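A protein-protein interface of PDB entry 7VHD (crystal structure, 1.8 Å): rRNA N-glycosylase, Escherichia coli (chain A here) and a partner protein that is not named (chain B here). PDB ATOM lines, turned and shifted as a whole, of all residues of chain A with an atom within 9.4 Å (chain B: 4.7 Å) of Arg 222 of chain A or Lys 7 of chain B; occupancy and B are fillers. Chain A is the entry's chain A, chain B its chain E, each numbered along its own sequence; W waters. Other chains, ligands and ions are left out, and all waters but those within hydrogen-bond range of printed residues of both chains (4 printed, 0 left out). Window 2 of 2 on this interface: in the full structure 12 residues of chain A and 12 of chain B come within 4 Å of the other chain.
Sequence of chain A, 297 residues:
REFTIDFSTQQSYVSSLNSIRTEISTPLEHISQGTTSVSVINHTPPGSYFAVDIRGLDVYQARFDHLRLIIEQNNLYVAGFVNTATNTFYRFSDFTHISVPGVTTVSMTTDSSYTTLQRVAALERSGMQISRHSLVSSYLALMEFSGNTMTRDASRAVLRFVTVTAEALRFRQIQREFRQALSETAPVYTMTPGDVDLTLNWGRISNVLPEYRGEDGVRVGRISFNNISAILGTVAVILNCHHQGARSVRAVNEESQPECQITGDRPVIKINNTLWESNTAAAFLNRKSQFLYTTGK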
ATOM      1  N   SER A 126     -17.937 -24.853  15.404  1.00  0.00           N
ATOM      2  CA  SER A 126     -18.302 -24.357  14.084  1.00  0.00           C
ATOM      3  C   SER A 126     -18.482 -25.546  13.150  1.00  0.00           C
ATOM      4  O   SER A 126     -17.521 -26.259  12.849  1.00  0.00           O
ATOM      5  CB  SER A 126     -17.237 -23.399  13.567  1.00  0.00           C
ATOM      6  OG  SER A 126     -17.702 -22.747  12.416  1.00  0.00           O
ATOM      7  N   PRO A 193     -20.668 -20.438  11.994  1.00  0.00           N
ATOM      8  CA  PRO A 193     -19.661 -19.512  12.517  1.00  0.00           C
ATOM      9  C   PRO A 193     -20.289 -18.290  13.147  1.00  0.00           C
ATOM     10  O   PRO A 193     -19.754 -17.772  14.131  1.00  0.00           O
ATOM     11  CB  PRO A 193     -18.833 -19.167  11.270  1.00  0.00           C
ATOM     12  CG  PRO A 193     -18.957 -20.395  10.415  1.00  0.00           C
ATOM     13  CD  PRO A 193     -20.368 -20.862  10.610  1.00  0.00           C
ATOM     14  N   GLY A 194     -21.410 -17.815  12.607  1.00  0.00           N
ATOM     15  CA  GLY A 194     -22.101 -16.692  13.223  1.00  0.00           C
ATOM     16  C   GLY A 194     -22.636 -17.032  14.601  1.00  0.00           C
ATOM     17  O   GLY A 194     -22.517 -16.230  15.533  1.00  0.00           O
ATOM     18  N   ASP A 195     -23.239 -18.216  14.746  1.00  0.00           N
ATOM     19  CA  ASP A 195     -23.661 -18.686  16.072  1.00  0.00           C
ATOM     20  C   ASP A 195     -22.479 -18.690  17.041  1.00  0.00           C
ATOM     21  O   ASP A 195     -22.571 -18.205  18.186  1.00  0.00           O
ATOM     22  CB  ASP A 195     -24.224 -20.113  15.976  1.00  0.00           C
ATOM     23  CG  ASP A 195     -25.531 -20.223  15.189  1.00  0.00           C
ATOM     24  OD1 ASP A 195     -26.259 -19.225  14.996  1.00  0.00           O
ATOM     25  OD2 ASP A 195     -25.827 -21.360  14.753  1.00  0.00           O
ATOM     26  N   VAL A 196     -21.356 -19.265  16.595  1.00  0.00           N
ATOM     27  CA  VAL A 196     -20.179 -19.352  17.454  1.00  0.00           C
ATOM     28  C   VAL A 196     -19.716 -17.953  17.861  1.00  0.00           C
ATOM     29  O   VAL A 196     -19.479 -17.680  19.046  1.00  0.00           O
ATOM     30  CB  VAL A 196     -19.065 -20.155  16.757  1.00  0.00           C
ATOM     31  CG1 VAL A 196     -17.768 -20.084  17.550  1.00  0.00           C
ATOM     32  CG2 VAL A 196     -19.487 -21.611  16.595  1.00  0.00           C
ATOM     33  N   ASP A 197     -19.574 -17.050  16.885  1.00  0.00           N
ATOM     34  CA  ASP A 197     -19.176 -15.679  17.190  1.00  0.00           C
ATOM     35  C   ASP A 197     -20.100 -15.037  18.211  1.00  0.00           C
ATOM     36  O   ASP A 197     -19.638 -14.321  19.110  1.00  0.00           O
ATOM     37  CB  ASP A 197     -19.147 -14.819  15.922  1.00  0.00           C
ATOM     38  CG  ASP A 197     -17.779 -14.788  15.277  1.00  0.00           C
ATOM     39  OD1 ASP A 197     -16.816 -15.215  15.944  1.00  0.00           O
ATOM     40  OD2 ASP A 197     -17.658 -14.284  14.137  1.00  0.00           O
ATOM     41  N   LEU A 198     -21.413 -15.247  18.072  1.00  0.00           N
ATOM     42  CA  LEU A 198     -22.328 -14.702  19.066  1.00  0.00           C
ATOM     43  C   LEU A 198     -21.939 -15.172  20.455  1.00  0.00           C
ATOM     44  O   LEU A 198     -21.790 -14.360  21.379  1.00  0.00           O
ATOM     45  CB  LEU A 198     -23.771 -15.107  18.756  1.00  0.00           C
ATOM     46  CG  LEU A 198     -24.522 -14.252  17.747  1.00  0.00           C
ATOM     47  CD1 LEU A 198     -25.863 -14.898  17.475  1.00  0.00           C
ATOM     48  CD2 LEU A 198     -24.706 -12.844  18.307  1.00  0.00           C
ATOM     49  N   LEU A 200     -19.152 -16.204  21.582  1.00  0.00           N
ATOM     50  CA  LEU A 200     -17.874 -15.664  22.037  1.00  0.00           C
ATOM     51  C   LEU A 200     -17.965 -14.186  22.386  1.00  0.00           C
ATOM     52  O   LEU A 200     -17.105 -13.673  23.110  1.00  0.00           O
ATOM     53  CB  LEU A 200     -16.816 -15.875  20.963  1.00  0.00           C
ATOM     54  CG  LEU A 200     -16.578 -17.343  20.621  1.00  0.00           C
ATOM     55  CD1 LEU A 200     -15.727 -17.432  19.352  1.00  0.00           C
ATOM     56  CD2 LEU A 200     -15.921 -18.059  21.793  1.00  0.00           C
ATOM     57  N   ASN A 201     -18.974 -13.482  21.879  1.00  0.00           N
ATOM     58  CA  ASN A 201     -19.084 -12.048  22.110  1.00  0.00           C
ATOM     59  C   ASN A 201     -20.146 -11.695  23.140  1.00  0.00           C
ATOM     60  O   ASN A 201     -20.546 -10.534  23.226  1.00  0.00           O
ATOM     61  CB  ASN A 201     -19.369 -11.335  20.794  1.00  0.00           C
ATOM     62  CG  ASN A 201     -18.130 -11.202  19.945  1.00  0.00           C
ATOM     63  OD1 ASN A 201     -17.378 -10.246  20.087  1.00  0.00           O
ATOM     64  ND2 ASN A 201     -17.886 -12.195  19.091  1.00  0.00           N
ATOM     65  N   ARG A 204     -19.184  -8.935  25.669  1.00  0.00           N
ATOM     66  CA  ARG A 204     -19.061  -7.632  25.024  1.00  0.00           C
ATOM     67  C   ARG A 204     -20.436  -7.066  24.671  1.00  0.00           C
ATOM     68  O   ARG A 204     -20.727  -5.878  24.917  1.00  0.00           O
ATOM     69  CB  ARG A 204     -18.169  -7.764  23.794  1.00  0.00           C
ATOM     70  CG  ARG A 204     -16.723  -8.163  24.166  1.00  0.00           C
ATOM     71  CD  ARG A 204     -15.932  -8.585  22.934  1.00  0.00           C
ATOM     72  NE  ARG A 204     -15.589  -7.443  22.091  1.00  0.00           N
ATOM     73  CZ  ARG A 204     -14.945  -7.543  20.936  1.00  0.00           C
ATOM     74  NH1 ARG A 204     -14.561  -8.720  20.460  1.00  0.00           N
ATOM     75  NH2 ARG A 204     -14.688  -6.438  20.238  1.00  0.00           N
ATOM     76  N   ILE A 205     -21.298  -7.916  24.111  1.00  0.00           N
ATOM     77  CA  ILE A 205     -22.669  -7.516  23.808  1.00  0.00           C
ATOM     78  C   ILE A 205     -23.366  -7.046  25.073  1.00  0.00           C
ATOM     79  O   ILE A 205     -24.073  -6.028  25.075  1.00  0.00           O
ATOM     80  CB  ILE A 205     -23.429  -8.683  23.149  1.00  0.00           C
ATOM     81  CG1 ILE A 205     -22.902  -8.948  21.737  1.00  0.00           C
ATOM     82  CG2 ILE A 205     -24.942  -8.389  23.112  1.00  0.00           C
ATOM     83  CD1 ILE A 205     -23.336 -10.301  21.147  1.00  0.00           C
ATOM     84  N   VAL A 218     -26.032  -1.186  15.989  1.00  0.00           N
ATOM     85  CA  VAL A 218     -25.165  -1.569  17.096  1.00  0.00           C
ATOM     86  C   VAL A 218     -24.027  -2.377  16.501  1.00  0.00           C
ATOM     87  O   VAL A 218     -24.262  -3.292  15.709  1.00  0.00           O
ATOM     88  CB  VAL A 218     -25.898  -2.398  18.171  1.00  0.00           C
ATOM     89  CG1 VAL A 218     -24.926  -2.828  19.268  1.00  0.00           C
ATOM     90  CG2 VAL A 218     -27.051  -1.607  18.756  1.00  0.00           C
ATOM     91  N   ARG A 219     -22.795  -2.040  16.872  1.00  0.00           N
ATOM     92  CA  ARG A 219     -21.618  -2.728  16.365  1.00  0.00           C
ATOM     93  C   ARG A 219     -20.764  -3.107  17.561  1.00  0.00           C
ATOM     94  O   ARG A 219     -20.358  -2.235  18.331  1.00  0.00           O
ATOM     95  CB  ARG A 219     -20.842  -1.842  15.384  1.00  0.00           C
ATOM     96  CG  ARG A 219     -21.619  -1.518  14.108  1.00  0.00           C
ATOM     97  CD  ARG A 219     -21.676  -2.727  13.170  1.00  0.00           C
ATOM     98  NE  ARG A 219     -20.408  -2.897  12.464  1.00  0.00           N
ATOM     99  CZ  ARG A 219     -19.482  -3.805  12.753  1.00  0.00           C
ATOM    100  NH1 ARG A 219     -19.683  -4.738  13.676  1.00  0.00           N
ATOM    101  NH2 ARG A 219     -18.322  -3.782  12.096  1.00  0.00           N
ATOM    102  N   VAL A 220     -20.518  -4.400  17.726  1.00  0.00           N
ATOM    103  CA  VAL A 220     -19.733  -4.934  18.829  1.00  0.00           C
ATOM    104  C   VAL A 220     -18.754  -5.911  18.198  1.00  0.00           C
ATOM    105  O   VAL A 220     -19.119  -7.050  17.898  1.00  0.00           O
ATOM    106  CB  VAL A 220     -20.602  -5.631  19.883  1.00  0.00           C
ATOM    107  CG1 VAL A 220     -19.726  -6.237  20.981  1.00  0.00           C
ATOM    108  CG2 VAL A 220     -21.620  -4.653  20.477  1.00  0.00           C
ATOM    109  N   GLY A 221     -17.511  -5.481  17.999  1.00  0.00           N
ATOM    110  CA  GLY A 221     -16.558  -6.317  17.287  1.00  0.00           C
ATOM    111  C   GLY A 221     -17.096  -6.800  15.956  1.00  0.00           C
ATOM    112  O   GLY A 221     -17.467  -5.997  15.090  1.00  0.00           O
ATOM    113  N   ARG A 222     -17.183  -8.121  15.791  1.00  0.00           N
ATOM    114  CA  ARG A 222     -17.665  -8.705  14.542  1.00  0.00           C
ATOM    115  C   ARG A 222     -19.186  -8.742  14.432  1.00  0.00           C
ATOM    116  O   ARG A 222     -19.703  -9.144  13.381  1.00  0.00           O
ATOM    117  CB  ARG A 222     -17.107 -10.126  14.394  1.00  0.00           C
ATOM    118  CG  ARG A 222     -15.574 -10.186  14.364  1.00  0.00           C
ATOM    119  CD  ARG A 222     -15.046 -11.555  14.750  1.00  0.00           C
ATOM    120  NE  ARG A 222     -15.432 -12.626  13.832  1.00  0.00           N
ATOM    121  CZ  ARG A 222     -14.814 -12.924  12.694  1.00  0.00           C
ATOM    122  NH1 ARG A 222     -13.823 -12.175  12.219  1.00  0.00           N
ATOM    123  NH2 ARG A 222     -15.188 -14.010  12.019  1.00  0.00           N
ATOM    124  N   ILE A 223     -19.898  -8.307  15.464  1.00  0.00           N
ATOM    125  CA  ILE A 223     -21.349  -8.437  15.571  1.00  0.00           C
ATOM    126  C   ILE A 223     -21.974  -7.126  15.132  1.00  0.00           C
ATOM    127  O   ILE A 223     -21.532  -6.052  15.561  1.00  0.00           O
ATOM    128  CB  ILE A 223     -21.772  -8.775  17.015  1.00  0.00           C
ATOM    129  CG1 ILE A 223     -20.968  -9.950  17.604  1.00  0.00           C
ATOM    130  CG2 ILE A 223     -23.275  -9.044  17.100  1.00  0.00           C
ATOM    131  CD1 ILE A 223     -21.104 -11.256  16.837  1.00  0.00           C
ATOM    132  N   SER A 224     -22.999  -7.201  14.280  1.00  0.00           N
ATOM    133  CA  SER A 224     -23.724  -6.013  13.851  1.00  0.00           C
ATOM    134  C   SER A 224     -25.220  -6.277  13.941  1.00  0.00           C
ATOM    135  O   SER A 224     -25.695  -7.335  13.516  1.00  0.00           O
ATOM    136  CB  SER A 224     -23.368  -5.608  12.415  1.00  0.00           C
ATOM    137  OG  SER A 224     -23.150  -6.743  11.596  1.00  0.00           O
ATOM    138  N   PHE A 225     -25.948  -5.302  14.482  1.00  0.00           N
ATOM    139  CA  PHE A 225     -27.408  -5.303  14.500  1.00  0.00           C
ATOM    140  C   PHE A 225     -27.891  -4.025  13.833  1.00  0.00           C
ATOM    141  O   PHE A 225     -27.392  -2.938  14.145  1.00  0.00           O
ATOM    142  CB  PHE A 225     -27.950  -5.369  15.931  1.00  0.00           C
ATOM    143  CG  PHE A 225     -27.440  -6.528  16.724  1.00  0.00           C
ATOM    144  CD1 PHE A 225     -27.569  -7.822  16.253  1.00  0.00           C
ATOM    145  CD2 PHE A 225     -26.837  -6.329  17.951  1.00  0.00           C
ATOM    146  CE1 PHE A 225     -27.094  -8.893  16.991  1.00  0.00           C
ATOM    147  CE2 PHE A 225     -26.364  -7.405  18.697  1.00  0.00           C
ATOM    148  CZ  PHE A 225     -26.500  -8.681  18.216  1.00  0.00           C
ATOM    149  N   TRP A 276     -21.384   1.991  18.842  1.00  0.00           N
ATOM    150  CA  TRP A 276     -20.184   1.167  18.758  1.00  0.00           C
ATOM    151  C   TRP A 276     -19.688   0.793  20.145  1.00  0.00           C
ATOM    152  O   TRP A 276     -19.641   1.634  21.042  1.00  0.00           O
ATOM    153  CB  TRP A 276     -19.045   1.905  18.044  1.00  0.00           C
ATOM    154  CG  TRP A 276     -19.224   2.013  16.573  1.00  0.00           C
ATOM    155  CD1 TRP A 276     -19.982   2.928  15.894  1.00  0.00           C
ATOM    156  CD2 TRP A 276     -18.646   1.158  15.593  1.00  0.00           C
ATOM    157  NE1 TRP A 276     -19.911   2.688  14.544  1.00  0.00           N
ATOM    158  CE2 TRP A 276     -19.088   1.609  14.333  1.00  0.00           C
ATOM    159  CE3 TRP A 276     -17.795   0.051  15.656  1.00  0.00           C
ATOM    160  CZ2 TRP A 276     -18.703   0.996  13.149  1.00  0.00           C
ATOM    161  CZ3 TRP A 276     -17.414  -0.550  14.480  1.00  0.00           C
ATOM    162  CH2 TRP A 276     -17.874  -0.081  13.243  1.00  0.00           C
ATOM    163  N   GLU A 277     -19.295  -0.464  20.312  1.00  0.00           N
ATOM    164  CA  GLU A 277     -18.394  -0.796  21.401  1.00  0.00           C
ATOM    165  C   GLU A 277     -17.143   0.063  21.263  1.00  0.00           C
ATOM    166  O   GLU A 277     -16.482   0.035  20.219  1.00  0.00           O
ATOM    167  CB  GLU A 277     -18.032  -2.275  21.357  1.00  0.00           C
ATOM    168  CG  GLU A 277     -17.176  -2.682  22.547  1.00  0.00           C
ATOM    169  CD  GLU A 277     -16.414  -3.956  22.280  1.00  0.00           C
ATOM    170  OE1 GLU A 277     -15.586  -3.971  21.343  1.00  0.00           O
ATOM    171  OE2 GLU A 277     -16.651  -4.945  23.003  1.00  0.00           O
ATOM    172  N   THR A 280     -13.899  -1.514  20.044  1.00  0.00           N
ATOM    173  CA  THR A 280     -13.809  -1.852  18.623  1.00  0.00           C
ATOM    174  C   THR A 280     -13.316  -0.656  17.807  1.00  0.00           C
ATOM    175  O   THR A 280     -12.392  -0.770  16.972  1.00  0.00           O
ATOM    176  CB  THR A 280     -15.172  -2.335  18.112  1.00  0.00           C
ATOM    177  OG1 THR A 280     -15.543  -3.548  18.784  1.00  0.00           O
ATOM    178  CG2 THR A 280     -15.152  -2.577  16.609  1.00  0.00           C
ATOM    179  N   GLY B   6     -15.332 -14.197   2.715  1.00  0.00           N
ATOM    180  CA  GLY B   6     -15.878 -14.473   4.027  1.00  0.00           C
ATOM    181  C   GLY B   6     -15.244 -13.579   5.067  1.00  0.00           C
ATOM    182  O   GLY B   6     -14.420 -12.723   4.763  1.00  0.00           O
ATOM    183  N   LYS B   7     -15.663 -13.794   6.309  1.00  0.00           N
ATOM    184  CA  LYS B   7     -15.010 -13.123   7.421  1.00  0.00           C
ATOM    185  C   LYS B   7     -13.658 -13.779   7.680  1.00  0.00           C
ATOM    186  O   LYS B   7     -13.426 -14.941   7.334  1.00  0.00           O
ATOM    187  CB  LYS B   7     -15.878 -13.188   8.675  1.00  0.00           C
ATOM    188  CG  LYS B   7     -17.209 -12.460   8.564  1.00  0.00           C
ATOM    189  CD  LYS B   7     -17.742 -12.102   9.943  1.00  0.00           C
ATOM    190  CE  LYS B   7     -19.173 -11.552   9.878  1.00  0.00           C
ATOM    191  NZ  LYS B   7     -19.652 -11.197  11.254  1.00  0.00           N
ATOM    192  N   ILE B   8     -12.750 -13.020   8.282  1.00  0.00           N
ATOM    193  CA  ILE B   8     -11.424 -13.546   8.588  1.00  0.00           C
ATOM    194  C   ILE B   8     -11.517 -14.394   9.849  1.00  0.00           C
ATOM    195  O   ILE B   8     -11.911 -13.904  10.909  1.00  0.00           O
ATOM    196  CB  ILE B   8     -10.398 -12.414   8.752  1.00  0.00           C
ATOM    197  CG1 ILE B   8     -10.153 -11.755   7.391  1.00  0.00           C
ATOM    198  CG2 ILE B   8      -9.114 -12.962   9.340  1.00  0.00           C
ATOM    199  CD1 ILE B   8      -9.442 -10.411   7.472  1.00  0.00           C
ATOM    200  N   GLU B   9     -11.152 -15.675   9.732  1.00  0.00           N
ATOM    201  CA  GLU B   9     -11.230 -16.586  10.870  1.00  0.00           C
ATOM    202  C   GLU B   9     -10.065 -16.391  11.832  1.00  0.00           C
ATOM    203  O   GLU B   9     -10.257 -16.416  13.053  1.00  0.00           O
ATOM    204  CB  GLU B   9     -11.263 -18.032  10.391  1.00  0.00           C
ATOM    205  CG  GLU B   9     -11.302 -18.997  11.558  1.00  0.00           C
ATOM    206  CD  GLU B   9     -11.342 -20.444  11.139  1.00  0.00           C
ATOM    207  OE1 GLU B   9     -11.497 -20.710   9.927  1.00  0.00           O
ATOM    208  OE2 GLU B   9     -11.227 -21.310  12.034  1.00  0.00           O
ATOM    209  N   LYS B  22      -6.947 -16.629   7.240  1.00  0.00           N
ATOM    210  CA  LYS B  22      -7.788 -17.758   6.875  1.00  0.00           C
ATOM    211  C   LYS B  22      -9.176 -17.221   6.581  1.00  0.00           C
ATOM    212  O   LYS B  22      -9.767 -16.525   7.408  1.00  0.00           O
ATOM    213  CB  LYS B  22      -7.831 -18.799   7.990  1.00  0.00           C
ATOM    214  CG  LYS B  22      -8.613 -20.034   7.600  1.00  0.00           C
ATOM    215  CD  LYS B  22      -8.286 -21.216   8.506  1.00  0.00           C
ATOM    216  CE  LYS B  22      -9.121 -22.443   8.119  1.00  0.00           C
ATOM    217  NZ  LYS B  22      -9.011 -23.527   9.134  1.00  0.00           N
ATOM    218  N   VAL B  23      -9.684 -17.525   5.396  1.00  0.00           N
ATOM    219  CA  VAL B  23     -10.977 -17.034   4.948  1.00  0.00           C
ATOM    220  C   VAL B  23     -11.683 -18.207   4.289  1.00  0.00           C
ATOM    221  O   VAL B  23     -11.122 -18.836   3.386  1.00  0.00           O
ATOM    222  CB  VAL B  23     -10.841 -15.856   3.968  1.00  0.00           C
ATOM    223  CG1 VAL B  23     -12.222 -15.347   3.541  1.00  0.00           C
ATOM    224  CG2 VAL B  23     -10.023 -14.724   4.591  1.00  0.00           C
ATOM    225  N   ASP B  24     -12.884 -18.529   4.766  1.00  0.00           N
ATOM    226  CA  ASP B  24     -13.696 -19.593   4.173  1.00  0.00           C
ATOM    227  C   ASP B  24     -12.913 -20.898   4.103  1.00  0.00           C
ATOM    228  O   ASP B  24     -12.885 -21.589   3.083  1.00  0.00           O
ATOM    229  CB  ASP B  24     -14.203 -19.187   2.789  1.00  0.00           C
ATOM    230  CG  ASP B  24     -15.296 -20.117   2.275  1.00  0.00           C
ATOM    231  OD1 ASP B  24     -15.990 -20.725   3.113  1.00  0.00           O
ATOM    232  OD2 ASP B  24     -15.450 -20.229   1.042  1.00  0.00           O
ATOM    233  N   GLN B  43     -10.819  -8.171  10.289  1.00  0.00           N
ATOM    234  CA  GLN B  43     -11.066  -9.311  11.166  1.00  0.00           C
ATOM    235  C   GLN B  43     -11.843  -8.900  12.411  1.00  0.00           C
ATOM    236  O   GLN B  43     -12.849  -9.528  12.771  1.00  0.00           O
ATOM    237  CB  GLN B  43      -9.734  -9.960  11.556  1.00  0.00           C
ATOM    238  CG  GLN B  43      -9.920 -11.151  12.482  1.00  0.00           C
ATOM    239  CD  GLN B  43      -8.587 -11.693  12.951  1.00  0.00           C
ATOM    240  OE1 GLN B  43      -7.534 -11.221  12.512  1.00  0.00           O
ATOM    241  NE2 GLN B  43      -8.622 -12.698  13.814  1.00  0.00           N
ATOM    242  N   LEU B  44     -11.393  -7.846  13.088  1.00  0.00           N
ATOM    243  CA  LEU B  44     -11.997  -7.516  14.369  1.00  0.00           C
ATOM    244  C   LEU B  44     -13.351  -6.840  14.224  1.00  0.00           C
ATOM    245  O   LEU B  44     -14.119  -6.830  15.192  1.00  0.00           O
ATOM    246  CB  LEU B  44     -11.044  -6.647  15.196  1.00  0.00           C
ATOM    247  CG  LEU B  44     -10.703  -5.208  14.819  1.00  0.00           C
ATOM    248  CD1 LEU B  44     -11.619  -4.256  15.573  1.00  0.00           C
ATOM    249  CD2 LEU B  44      -9.239  -4.936  15.164  1.00  0.00           C
ATOM    250  N   THR B  45     -13.665  -6.287  13.050  1.00  0.00           N
ATOM    251  CA  THR B  45     -14.969  -5.680  12.799  1.00  0.00           C
ATOM    252  C   THR B  45     -15.910  -6.585  12.026  1.00  0.00           C
ATOM    253  O   THR B  45     -17.059  -6.194  11.777  1.00  0.00           O
ATOM    254  CB  THR B  45     -14.815  -4.374  12.019  1.00  0.00           C
ATOM    255  OG1 THR B  45     -14.162  -4.648  10.771  1.00  0.00           O
ATOM    256  CG2 THR B  45     -14.024  -3.350  12.821  1.00  0.00           C
ATOM    257  N   GLY B  46     -15.450  -7.762  11.614  1.00  0.00           N
ATOM    258  CA  GLY B  46     -16.328  -8.672  10.911  1.00  0.00           C
ATOM    259  C   GLY B  46     -16.639  -8.284   9.488  1.00  0.00           C
ATOM    260  O   GLY B  46     -17.697  -8.663   8.963  1.00  0.00           O
ATOM    261  N   MET B  47     -15.755  -7.547   8.827  1.00  0.00           N
ATOM    262  CA  MET B  47     -16.023  -7.338   7.417  1.00  0.00           C
ATOM    263  C   MET B  47     -15.859  -8.613   6.605  1.00  0.00           C
ATOM    264  O   MET B  47     -15.145  -9.544   6.974  1.00  0.00           O
ATOM    265  CB  MET B  47     -15.197  -6.194   6.784  1.00  0.00           C
ATOM    266  CG  MET B  47     -14.916  -4.906   7.567  1.00  0.00           C
ATOM    267  SD  MET B  47     -13.682  -3.876   6.707  1.00  0.00           S
ATOM    268  CE  MET B  47     -14.748  -2.747   5.776  1.00  0.00           C
ATOM    269  N   THR B  48     -16.584  -8.648   5.492  1.00  0.00           N
ATOM    270  CA  THR B  48     -16.426  -9.688   4.494  1.00  0.00           C
ATOM    271  C   THR B  48     -15.275  -9.294   3.586  1.00  0.00           C
ATOM    272  O   THR B  48     -15.292  -8.216   2.973  1.00  0.00           O
ATOM    273  CB  THR B  48     -17.718  -9.860   3.696  1.00  0.00           C
ATOM    274  OG1 THR B  48     -18.741 -10.343   4.565  1.00  0.00           O
ATOM    275  CG2 THR B  48     -17.512 -10.846   2.549  1.00  0.00           C
HETATM  276  O   HOH W   1     -13.471  -7.641  17.783  1.00  0.00           O
HETATM  277  O   HOH W   2     -18.661  -5.328   9.288  1.00  0.00           O
HETATM  278  O   HOH W   3     -14.534 -16.236  10.235  1.00  0.00           O
HETATM  279  O   HOH W   4     -19.666 -13.309  13.049  1.00  0.00           O
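Printed residues of chain A that touch a printed residue of chain B: Arg 219, Gly 221, Arg 222 and Thr 280.
Of the 13 printed residues of chain B, 6 touch a printed residue of chain A.
Among the printed residues, merely in contact across the chains: Arg 222 of chain A with Gly 46 of chain B (3.7 Å), Arg 222 of chain A with Thr 45 of chain B (3.7 Å) and Thr 280 of chain A with Leu 44 of chain B (3.8 Å).
NH1 of Arg 219 of chain A is in hydrogen-bond range of O of Gly 221 of chain A (2.9 Å).
The guanidinium group (NE) of Arg 222 of chain A lies within salt-bridge range of the side-chain carboxylate (OD2) of Asp 197 of chain A, 2.8 Å away.
The backbone NH of Gly 221 of chain A sits at hydrogen-bond distance from the side-chain hydroxyl of Thr 280 of chain A (2.9 Å).
NH1 of Arg 219 of chain A is in hydrogen-bond range of O of Ile 223 of chain A.
OE1 of Glu 277 of chain A sits at hydrogen-bond distance from OG1 of Thr 280 of chain A (2.6 Å).
The side-chain hydroxyl (OG1) of Thr 280 of chain A is in hydrogen-bond range of the guanidinium group (NH2) of Arg 204 of chain A, 3.3 Å away.
Of the printed residues of chain B, Gly 221 of chain A touches Leu 44 (3.1 Å) and Thr 45 (3.3 Å).
Arg 222 of chain A touches six residues of chain B.
Of the printed residues of chain B, Thr 280 of chain A touches Leu 44 (3.8 Å).
No residue of chain A comes within 4 Å of Gly 6 of chain B.
Printed residues of chain A within 4 Å of Ile 8 of chain B: Arg 222.
Of the printed residues of chain A, Gln 43 of chain B touches Arg 222 (2.9 Å).
The nearest printed residue of chain B that does not touch Thr 280 of chain A is Thr 45 of chain B (4.03 Å).
O of Thr 45 of chain B lies within hydrogen-bond range of NH2 of Arg 219 of chain A (2.7 Å).
NH1 of Arg 222 of chain A sits at hydrogen-bond distance from O of Ile 8 of chain B.
The backbone NH (N) of Arg 222 of chain A sits at hydrogen-bond distance from the backbone carbonyl oxygen (O) of Leu 44 of chain B, 3.4 Å away.
The backbone carbonyl oxygen of Leu 44 of chain B lies close to the backbone carbonyl oxygen of Gly 221 of chain A (3.5 Å).
NZ of Lys 7 of chain B sits at hydrogen-bond distance from O of Arg 222 of chain A (3.0 Å).
The backbone carbonyl oxygen (O) of Thr 45 of chain B sits close to the backbone carbonyl oxygen (O) of Gly 221 of chain A, at 3.3 Å.
NH1 of Arg 222 of chain A lies within hydrogen-bond range of O of Gln 43 of chain B, 2.9 Å away.
Water W4 lies within hydrogen-bond range of the side-chain carboxylate (OD2) of Asp 197 of chain A and the side-chain amino group (NZ) of Lys 7 of chain B.
Water W1 lies within hydrogen-bond range of the backbone carbonyl oxygen (O) of Leu 44 of chain B (2.8 Å) and the guanidinium group (NH2) of Arg 204 of chain A (3.0 Å).
Water W3 lies within hydrogen-bond range of the guanidinium group (NH2) of Arg 222 of chain A (2.9 Å), the backbone carbonyl oxygen (O) of Lys 7 of chain B (3.4 Å) and the backbone NH (N) of Glu 9 of chain B (3.5 Å).
Water W2 lies within hydrogen-bond range of O of Thr 45 of chain B, NH2 of Arg 219 of chain A and O of Gly 46 of chain B.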
